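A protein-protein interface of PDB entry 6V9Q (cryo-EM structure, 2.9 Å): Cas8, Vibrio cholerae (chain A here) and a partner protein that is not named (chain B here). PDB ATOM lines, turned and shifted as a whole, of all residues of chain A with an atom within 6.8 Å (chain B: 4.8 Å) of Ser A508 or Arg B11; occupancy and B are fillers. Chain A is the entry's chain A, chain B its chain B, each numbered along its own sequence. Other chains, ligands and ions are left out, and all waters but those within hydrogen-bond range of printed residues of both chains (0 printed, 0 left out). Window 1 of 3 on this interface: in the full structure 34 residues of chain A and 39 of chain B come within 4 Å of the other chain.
OE2 of Glu B10 lies within salt-bridge range of NE of Arg A503 (3.6 Å).
The guanidinium group (NH2) of Arg B11 lies within hydrogen-bond range of the side-chain hydroxyl (OG) of Ser A508.
The side-chain hydroxyl (OG) of Ser A508 lies within hydrogen-bond range of the side-chain carboxylate (OD1) of Asp B14, 2.6 Å away.
The backbone carbonyl oxygen (O) of Pro B15 lies within hydrogen-bond range of the side-chain hydroxyl (OG) of Ser A508, 3.0 Å away.
The side-chain amino group (NZ) of Lys A510 lies within salt-bridge range of the side-chain carboxylate (OD2) of Asp B14, 3.7 Å away.
The backbone carbonyl oxygen of Pro B15 lies within hydrogen-bond range of the side-chain amino group of Lys A510, 3.3 Å away.
O of Lys A502 sits close to OD2 of Asp B14 (3.1 Å).
O of Lys A510 sits at hydrogen-bond distance from N of Arg A394 (3.0 Å).
The backbone NH (N) of Cys A396 lies within hydrogen-bond range of the backbone carbonyl oxygen (O) of Ser A508 (3.3 Å).
The backbone carbonyl oxygen (O) of Lys A502 lies within hydrogen-bond range of the backbone NH (N) of Ala A509, 3.5 Å away.
OD1 of Asp B14 lies within salt-bridge range of NH2 of Arg B11 (2.5 Å).
The backbone NH (N) of Ser B94 lies within hydrogen-bond range of the backbone carbonyl oxygen (O) of Ser B12.
The side-chain hydroxyl (OG) of Ser B94 lies within hydrogen-bond range of the backbone NH (N) of Glu B96, at 3.3 Å.
Among the printed residues, pairs that only touch across the chains: Lys A502 with Ser B94.
Of the printed residues of chain B, Lys A502 touches Asp B14 and Ser B94.
Of the printed residues of chain B, Lys A510 touches Asp B14 and Pro B15.
Printed residues of chain A within 4 Å of Glu B10: Arg A503 (3.6 Å).
Arg B11 touches just one residue of chain A: Ser A508.
Printed residues of chain A within 4 Å of Asp B14: Lys A502 (3.1 Å), Ser A508 (2.6 Å) and Lys A510 (3.0 Å).
Of the printed residues of chain A, Ser B94 touches Lys A502.
The nearest residue of chain A that does not touch Arg B11 is Arg A506 (5.6 Å).
The nearest printed residue of chain B that does not touch Arg A503 is Asp B14 (5.3 Å).
Of the 13 printed residues of chain B, 5 touch a printed residue of chain A.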
ATOM      1  N   ILE A 393     -22.043   7.440 -25.836  1.00  0.00           N
ATOM      2  CA  ILE A 393     -22.158   6.065 -25.375  1.00  0.00           C
ATOM      3  C   ILE A 393     -22.503   6.117 -23.891  1.00  0.00           C
ATOM      4  O   ILE A 393     -21.614   5.958 -23.050  1.00  0.00           O
ATOM      5  CB  ILE A 393     -20.852   5.289 -25.576  1.00  0.00           C
ATOM      6  CG1 ILE A 393     -20.182   5.626 -26.910  1.00  0.00           C
ATOM      7  CG2 ILE A 393     -21.125   3.803 -25.513  1.00  0.00           C
ATOM      8  CD1 ILE A 393     -20.915   5.177 -28.118  1.00  0.00           C
ATOM      9  N   ARG A 394     -23.775   6.293 -23.552  1.00  0.00           N
ATOM     10  CA  ARG A 394     -24.186   6.435 -22.157  1.00  0.00           C
ATOM     11  C   ARG A 394     -24.128   5.072 -21.474  1.00  0.00           C
ATOM     12  O   ARG A 394     -24.912   4.179 -21.802  1.00  0.00           O
ATOM     13  CB  ARG A 394     -25.580   7.055 -22.060  1.00  0.00           C
ATOM     14  CG  ARG A 394     -26.093   7.308 -20.646  1.00  0.00           C
ATOM     15  CD  ARG A 394     -27.097   6.246 -20.217  1.00  0.00           C
ATOM     16  NE  ARG A 394     -27.597   6.453 -18.864  1.00  0.00           N
ATOM     17  CZ  ARG A 394     -28.639   7.217 -18.568  1.00  0.00           C
ATOM     18  NH1 ARG A 394     -29.035   7.345 -17.311  1.00  0.00           N
ATOM     19  NH2 ARG A 394     -29.288   7.851 -19.530  1.00  0.00           N
ATOM     20  N   VAL A 395     -23.209   4.923 -20.521  1.00  0.00           N
ATOM     21  CA  VAL A 395     -23.009   3.681 -19.777  1.00  0.00           C
ATOM     22  C   VAL A 395     -23.634   3.828 -18.399  1.00  0.00           C
ATOM     23  O   VAL A 395     -23.353   4.797 -17.686  1.00  0.00           O
ATOM     24  CB  VAL A 395     -21.518   3.325 -19.677  1.00  0.00           C
ATOM     25  CG1 VAL A 395     -21.289   2.227 -18.671  1.00  0.00           C
ATOM     26  CG2 VAL A 395     -21.045   2.837 -20.992  1.00  0.00           C
ATOM     27  N   CYS A 396     -24.495   2.880 -18.021  1.00  0.00           N
ATOM     28  CA  CYS A 396     -25.168   2.996 -16.734  1.00  0.00           C
ATOM     29  C   CYS A 396     -24.368   2.462 -15.554  1.00  0.00           C
ATOM     30  O   CYS A 396     -23.935   3.249 -14.719  1.00  0.00           O
ATOM     31  CB  CYS A 396     -26.527   2.309 -16.796  1.00  0.00           C
ATOM     32  SG  CYS A 396     -27.692   3.239 -17.779  1.00  0.00           S
ATOM     33  N   GLY A 397     -24.145   1.160 -15.443  1.00  0.00           N
ATOM     34  CA  GLY A 397     -23.387   0.772 -14.271  1.00  0.00           C
ATOM     35  C   GLY A 397     -22.055   0.121 -14.538  1.00  0.00           C
ATOM     36  O   GLY A 397     -21.976  -1.102 -14.645  1.00  0.00           O
ATOM     37  N   ALA A 398     -20.987   0.902 -14.476  1.00  0.00           N
ATOM     38  CA  ALA A 398     -19.654   0.419 -14.778  1.00  0.00           C
ATOM     39  C   ALA A 398     -18.947   0.120 -13.469  1.00  0.00           C
ATOM     40  O   ALA A 398     -19.488   0.352 -12.393  1.00  0.00           O
ATOM     41  CB  ALA A 398     -18.866   1.436 -15.608  1.00  0.00           C
ATOM     42  N   LYS A 502     -22.392  -4.184 -26.279  1.00  0.00           N
ATOM     43  CA  LYS A 502     -23.424  -3.712 -25.376  1.00  0.00           C
ATOM     44  C   LYS A 502     -22.966  -3.601 -23.936  1.00  0.00           C
ATOM     45  O   LYS A 502     -23.808  -3.461 -23.046  1.00  0.00           O
ATOM     46  CB  LYS A 502     -24.641  -4.630 -25.464  1.00  0.00           C
ATOM     47  CG  LYS A 502     -25.285  -4.550 -26.817  1.00  0.00           C
ATOM     48  CD  LYS A 502     -26.559  -5.336 -26.916  1.00  0.00           C
ATOM     49  CE  LYS A 502     -27.143  -5.138 -28.296  1.00  0.00           C
ATOM     50  NZ  LYS A 502     -28.461  -5.776 -28.473  1.00  0.00           N
ATOM     51  N   ARG A 503     -21.665  -3.651 -23.682  1.00  0.00           N
ATOM     52  CA  ARG A 503     -21.142  -3.525 -22.333  1.00  0.00           C
ATOM     53  C   ARG A 503     -19.818  -2.779 -22.371  1.00  0.00           C
ATOM     54  O   ARG A 503     -19.031  -2.951 -23.304  1.00  0.00           O
ATOM     55  CB  ARG A 503     -21.011  -4.901 -21.676  1.00  0.00           C
ATOM     56  CG  ARG A 503     -20.115  -5.874 -22.403  1.00  0.00           C
ATOM     57  CD  ARG A 503     -20.130  -7.228 -21.738  1.00  0.00           C
ATOM     58  NE  ARG A 503     -19.303  -8.207 -22.434  1.00  0.00           N
ATOM     59  CZ  ARG A 503     -18.018  -8.411 -22.173  1.00  0.00           C
ATOM     60  NH1 ARG A 503     -17.414  -7.705 -21.231  1.00  0.00           N
ATOM     61  NH2 ARG A 503     -17.338  -9.324 -22.847  1.00  0.00           N
ATOM     62  N   LEU A 504     -19.601  -1.914 -21.384  1.00  0.00           N
ATOM     63  CA  LEU A 504     -18.332  -1.218 -21.184  1.00  0.00           C
ATOM     64  C   LEU A 504     -17.984  -1.335 -19.710  1.00  0.00           C
ATOM     65  O   LEU A 504     -18.460  -0.535 -18.900  1.00  0.00           O
ATOM     66  CB  LEU A 504     -18.418   0.244 -21.629  1.00  0.00           C
ATOM     67  CG  LEU A 504     -17.195   1.180 -21.691  1.00  0.00           C
ATOM     68  CD1 LEU A 504     -16.880   1.916 -20.404  1.00  0.00           C
ATOM     69  CD2 LEU A 504     -15.979   0.411 -22.108  1.00  0.00           C
ATOM     70  N   ALA A 505     -17.150  -2.328 -19.387  1.00  0.00           N
ATOM     71  CA  ALA A 505     -16.762  -2.681 -18.020  1.00  0.00           C
ATOM     72  C   ALA A 505     -17.986  -2.896 -17.137  1.00  0.00           C
ATOM     73  O   ALA A 505     -18.230  -2.138 -16.201  1.00  0.00           O
ATOM     74  CB  ALA A 505     -15.823  -1.635 -17.419  1.00  0.00           C
ATOM     75  N   ARG A 506     -18.783  -3.911 -17.501  1.00  0.00           N
ATOM     76  CA  ARG A 506     -20.005  -4.382 -16.843  1.00  0.00           C
ATOM     77  C   ARG A 506     -21.180  -3.409 -16.935  1.00  0.00           C
ATOM     78  O   ARG A 506     -22.175  -3.591 -16.231  1.00  0.00           O
ATOM     79  CB  ARG A 506     -19.774  -4.700 -15.361  1.00  0.00           C
ATOM     80  CG  ARG A 506     -18.758  -5.751 -15.017  1.00  0.00           C
ATOM     81  CD  ARG A 506     -18.713  -5.797 -13.510  1.00  0.00           C
ATOM     82  NE  ARG A 506     -17.681  -6.646 -12.938  1.00  0.00           N
ATOM     83  CZ  ARG A 506     -17.407  -6.680 -11.640  1.00  0.00           C
ATOM     84  NH1 ARG A 506     -18.081  -5.904 -10.810  1.00  0.00           N
ATOM     85  NH2 ARG A 506     -16.461  -7.479 -11.171  1.00  0.00           N
ATOM     86  N   GLY A 507     -21.100  -2.384 -17.777  1.00  0.00           N
ATOM     87  CA  GLY A 507     -22.152  -1.388 -17.813  1.00  0.00           C
ATOM     88  C   GLY A 507     -22.863  -1.308 -19.146  1.00  0.00           C
ATOM     89  O   GLY A 507     -22.259  -1.410 -20.203  1.00  0.00           O
ATOM     90  N   SER A 508     -24.171  -1.071 -19.084  1.00  0.00           N
ATOM     91  CA  SER A 508     -25.025  -1.037 -20.266  1.00  0.00           C
ATOM     92  C   SER A 508     -24.689   0.170 -21.131  1.00  0.00           C
ATOM     93  O   SER A 508     -25.090   1.293 -20.816  1.00  0.00           O
ATOM     94  CB  SER A 508     -26.497  -0.985 -19.869  1.00  0.00           C
ATOM     95  OG  SER A 508     -26.880  -2.159 -19.184  1.00  0.00           O
ATOM     96  N   ALA A 509     -23.980  -0.071 -22.226  1.00  0.00           N
ATOM     97  CA  ALA A 509     -23.587   0.965 -23.169  1.00  0.00           C
ATOM     98  C   ALA A 509     -24.630   1.064 -24.270  1.00  0.00           C
ATOM     99  O   ALA A 509     -24.953   0.060 -24.909  1.00  0.00           O
ATOM    100  CB  ALA A 509     -22.219   0.658 -23.773  1.00  0.00           C
ATOM    101  N   LYS A 510     -25.157   2.267 -24.488  1.00  0.00           N
ATOM    102  CA  LYS A 510     -26.191   2.491 -25.487  1.00  0.00           C
ATOM    103  C   LYS A 510     -25.988   3.832 -26.171  1.00  0.00           C
ATOM    104  O   LYS A 510     -25.398   4.756 -25.613  1.00  0.00           O
ATOM    105  CB  LYS A 510     -27.593   2.455 -24.874  1.00  0.00           C
ATOM    106  CG  LYS A 510     -28.064   1.087 -24.459  1.00  0.00           C
ATOM    107  CD  LYS A 510     -29.399   1.139 -23.793  1.00  0.00           C
ATOM    108  CE  LYS A 510     -29.882  -0.250 -23.512  1.00  0.00           C
ATOM    109  NZ  LYS A 510     -28.964  -0.911 -22.561  1.00  0.00           N
ATOM    110  N   TYR B   9     -23.448 -18.004 -20.031  1.00  0.00           N
ATOM    111  CA  TYR B   9     -24.033 -17.310 -21.170  1.00  0.00           C
ATOM    112  C   TYR B   9     -24.157 -15.830 -20.839  1.00  0.00           C
ATOM    113  O   TYR B   9     -24.262 -15.439 -19.677  1.00  0.00           O
ATOM    114  CB  TYR B   9     -25.442 -17.818 -21.598  1.00  0.00           C
ATOM    115  CG  TYR B   9     -25.627 -19.279 -22.019  1.00  0.00           C
ATOM    116  CD1 TYR B   9     -24.599 -20.190 -21.953  1.00  0.00           C
ATOM    117  CD2 TYR B   9     -26.831 -19.713 -22.557  1.00  0.00           C
ATOM    118  CE1 TYR B   9     -24.758 -21.480 -22.311  1.00  0.00           C
ATOM    119  CE2 TYR B   9     -27.002 -21.033 -22.945  1.00  0.00           C
ATOM    120  CZ  TYR B   9     -25.947 -21.905 -22.814  1.00  0.00           C
ATOM    121  OH  TYR B   9     -26.018 -23.226 -23.165  1.00  0.00           O
ATOM    122  N   GLU B  10     -24.133 -15.001 -21.875  1.00  0.00           N
ATOM    123  CA  GLU B  10     -24.466 -13.606 -21.674  1.00  0.00           C
ATOM    124  C   GLU B  10     -25.974 -13.417 -21.631  1.00  0.00           C
ATOM    125  O   GLU B  10     -26.750 -14.287 -22.032  1.00  0.00           O
ATOM    126  CB  GLU B  10     -23.882 -12.729 -22.773  1.00  0.00           C
ATOM    127  CG  GLU B  10     -22.398 -12.533 -22.707  1.00  0.00           C
ATOM    128  CD  GLU B  10     -21.911 -11.588 -23.778  1.00  0.00           C
ATOM    129  OE1 GLU B  10     -22.727 -11.205 -24.640  1.00  0.00           O
ATOM    130  OE2 GLU B  10     -20.722 -11.218 -23.760  1.00  0.00           O
ATOM    131  N   ARG B  11     -26.388 -12.252 -21.148  1.00  0.00           N
ATOM    132  CA  ARG B  11     -27.804 -11.946 -21.074  1.00  0.00           C
ATOM    133  C   ARG B  11     -28.312 -11.415 -22.407  1.00  0.00           C
ATOM    134  O   ARG B  11     -27.582 -10.781 -23.171  1.00  0.00           O
ATOM    135  CB  ARG B  11     -28.088 -10.942 -19.959  1.00  0.00           C
ATOM    136  CG  ARG B  11     -27.455  -9.594 -20.133  1.00  0.00           C
ATOM    137  CD  ARG B  11     -27.845  -8.683 -19.006  1.00  0.00           C
ATOM    138  NE  ARG B  11     -27.285  -7.354 -19.170  1.00  0.00           N
ATOM    139  CZ  ARG B  11     -27.553  -6.337 -18.366  1.00  0.00           C
ATOM    140  NH1 ARG B  11     -28.379  -6.494 -17.347  1.00  0.00           N
ATOM    141  NH2 ARG B  11     -27.002  -5.157 -18.590  1.00  0.00           N
ATOM    142  N   SER B  12     -29.580 -11.697 -22.687  1.00  0.00           N
ATOM    143  CA  SER B  12     -30.202 -11.307 -23.942  1.00  0.00           C
ATOM    144  C   SER B  12     -31.038 -10.045 -23.827  1.00  0.00           C
ATOM    145  O   SER B  12     -31.451  -9.505 -24.852  1.00  0.00           O
ATOM    146  CB  SER B  12     -31.082 -12.441 -24.469  1.00  0.00           C
ATOM    147  OG  SER B  12     -30.311 -13.593 -24.731  1.00  0.00           O
ATOM    148  N   ILE B  13     -31.300  -9.568 -22.617  1.00  0.00           N
ATOM    149  CA  ILE B  13     -32.094  -8.371 -22.379  1.00  0.00           C
ATOM    150  C   ILE B  13     -31.243  -7.397 -21.584  1.00  0.00           C
ATOM    151  O   ILE B  13     -30.722  -7.751 -20.523  1.00  0.00           O
ATOM    152  CB  ILE B  13     -33.394  -8.707 -21.633  1.00  0.00           C
ATOM    153  CG1 ILE B  13     -34.270  -9.594 -22.501  1.00  0.00           C
ATOM    154  CG2 ILE B  13     -34.138  -7.459 -21.247  1.00  0.00           C
ATOM    155  CD1 ILE B  13     -35.412 -10.172 -21.777  1.00  0.00           C
ATOM    156  N   ASP B  14     -31.111  -6.174 -22.088  1.00  0.00           N
ATOM    157  CA  ASP B  14     -30.160  -5.203 -21.552  1.00  0.00           C
ATOM    158  C   ASP B  14     -30.864  -3.883 -21.260  1.00  0.00           C
ATOM    159  O   ASP B  14     -30.998  -3.039 -22.161  1.00  0.00           O
ATOM    160  CB  ASP B  14     -29.018  -4.995 -22.535  1.00  0.00           C
ATOM    161  CG  ASP B  14     -27.820  -4.314 -21.912  1.00  0.00           C
ATOM    162  OD1 ASP B  14     -27.828  -4.065 -20.688  1.00  0.00           O
ATOM    163  OD2 ASP B  14     -26.868  -4.012 -22.658  1.00  0.00           O
ATOM    164  N   PRO B  15     -31.325  -3.661 -20.030  1.00  0.00           N
ATOM    165  CA  PRO B  15     -31.988  -2.392 -19.707  1.00  0.00           C
ATOM    166  C   PRO B  15     -31.016  -1.281 -19.355  1.00  0.00           C
ATOM    167  O   PRO B  15     -29.801  -1.462 -19.450  1.00  0.00           O
ATOM    168  CB  PRO B  15     -32.853  -2.753 -18.499  1.00  0.00           C
ATOM    169  CG  PRO B  15     -32.945  -4.219 -18.516  1.00  0.00           C
ATOM    170  CD  PRO B  15     -31.641  -4.689 -19.035  1.00  0.00           C
ATOM    171  N   SER B  94     -30.849  -8.848 -27.525  1.00  0.00           N
ATOM    172  CA  SER B  94     -29.630  -9.045 -28.299  1.00  0.00           C
ATOM    173  C   SER B  94     -29.537 -10.386 -29.004  1.00  0.00           C
ATOM    174  O   SER B  94     -28.830 -10.470 -30.015  1.00  0.00           O
ATOM    175  CB  SER B  94     -28.397  -8.910 -27.403  1.00  0.00           C
ATOM    176  OG  SER B  94     -28.280 -10.013 -26.527  1.00  0.00           O
ATOM    177  N   GLU B  96     -28.007 -13.183 -27.527  1.00  0.00           N
ATOM    178  CA  GLU B  96     -26.835 -13.948 -27.129  1.00  0.00           C
ATOM    179  C   GLU B  96     -27.236 -15.308 -26.581  1.00  0.00           C
ATOM    180  O   GLU B  96     -26.422 -16.002 -25.966  1.00  0.00           O
ATOM    181  CB  GLU B  96     -26.024 -13.163 -26.103  1.00  0.00           C
ATOM    182  CG  GLU B  96     -25.453 -11.866 -26.649  1.00  0.00           C
ATOM    183  CD  GLU B  96     -24.353 -12.085 -27.676  1.00  0.00           C
ATOM    184  OE1 GLU B  96     -23.572 -13.050 -27.527  1.00  0.00           O
ATOM    185  OE2 GLU B  96     -24.277 -11.294 -28.640  1.00  0.00           O
ATOM    186  N   PHE B 262     -29.996  -2.788 -12.749  1.00  0.00           N
ATOM    187  CA  PHE B 262     -30.264  -4.140 -12.280  1.00  0.00           C
ATOM    188  C   PHE B 262     -31.634  -4.245 -11.633  1.00  0.00           C
ATOM    189  O   PHE B 262     -32.242  -5.318 -11.645  1.00  0.00           O
ATOM    190  CB  PHE B 262     -29.169  -4.551 -11.305  1.00  0.00           C
ATOM    191  CG  PHE B 262     -27.847  -4.786 -11.958  1.00  0.00           C
ATOM    192  CD1 PHE B 262     -27.777  -5.268 -13.250  1.00  0.00           C
ATOM    193  CD2 PHE B 262     -26.676  -4.440 -11.317  1.00  0.00           C
ATOM    194  CE1 PHE B 262     -26.564  -5.468 -13.862  1.00  0.00           C
ATOM    195  CE2 PHE B 262     -25.461  -4.624 -11.933  1.00  0.00           C
ATOM    196  CZ  PHE B 262     -25.406  -5.142 -13.203  1.00  0.00           C
ATOM    197  N   ILE B 342     -32.014 -16.795 -21.449  1.00  0.00           N
ATOM    198  CA  ILE B 342     -32.175 -15.385 -21.772  1.00  0.00           C
ATOM    199  C   ILE B 342     -31.597 -14.532 -20.654  1.00  0.00           C
ATOM    200  O   ILE B 342     -30.988 -13.485 -20.900  1.00  0.00           O
ATOM    201  CB  ILE B 342     -33.664 -15.095 -22.030  1.00  0.00           C
ATOM    202  CG1 ILE B 342     -34.137 -15.885 -23.242  1.00  0.00           C
ATOM    203  CG2 ILE B 342     -33.926 -13.625 -22.260  1.00  0.00           C
ATOM    204  CD1 ILE B 342     -35.618 -15.910 -23.392  1.00  0.00           C
ATOM    205  N   LYS B 343     -31.732 -14.991 -19.413  1.00  0.00           N
ATOM    206  CA  LYS B 343     -31.175 -14.278 -18.275  1.00  0.00           C
ATOM    207  C   LYS B 343     -29.660 -14.441 -18.190  1.00  0.00           C
ATOM    208  O   LYS B 343     -28.966 -13.522 -17.749  1.00  0.00           O
ATOM    209  CB  LYS B 343     -31.884 -14.767 -17.012  1.00  0.00           C
ATOM    210  CG  LYS B 343     -31.505 -14.100 -15.727  1.00  0.00           C
ATOM    211  CD  LYS B 343     -30.654 -15.023 -14.902  1.00  0.00           C
ATOM    212  CE  LYS B 343     -30.295 -14.377 -13.610  1.00  0.00           C
ATOM    213  NZ  LYS B 343     -31.490 -14.167 -12.767  1.00  0.00           N
ATOM    214  N   GLY B 344     -29.129 -15.578 -18.616  1.00  0.00           N
ATOM    215  CA  GLY B 344     -27.700 -15.792 -18.600  1.00  0.00           C
ATOM    216  C   GLY B 344     -27.203 -16.266 -17.250  1.00  0.00           C
ATOM    217  O   GLY B 344     -27.967 -16.491 -16.312  1.00  0.00           O
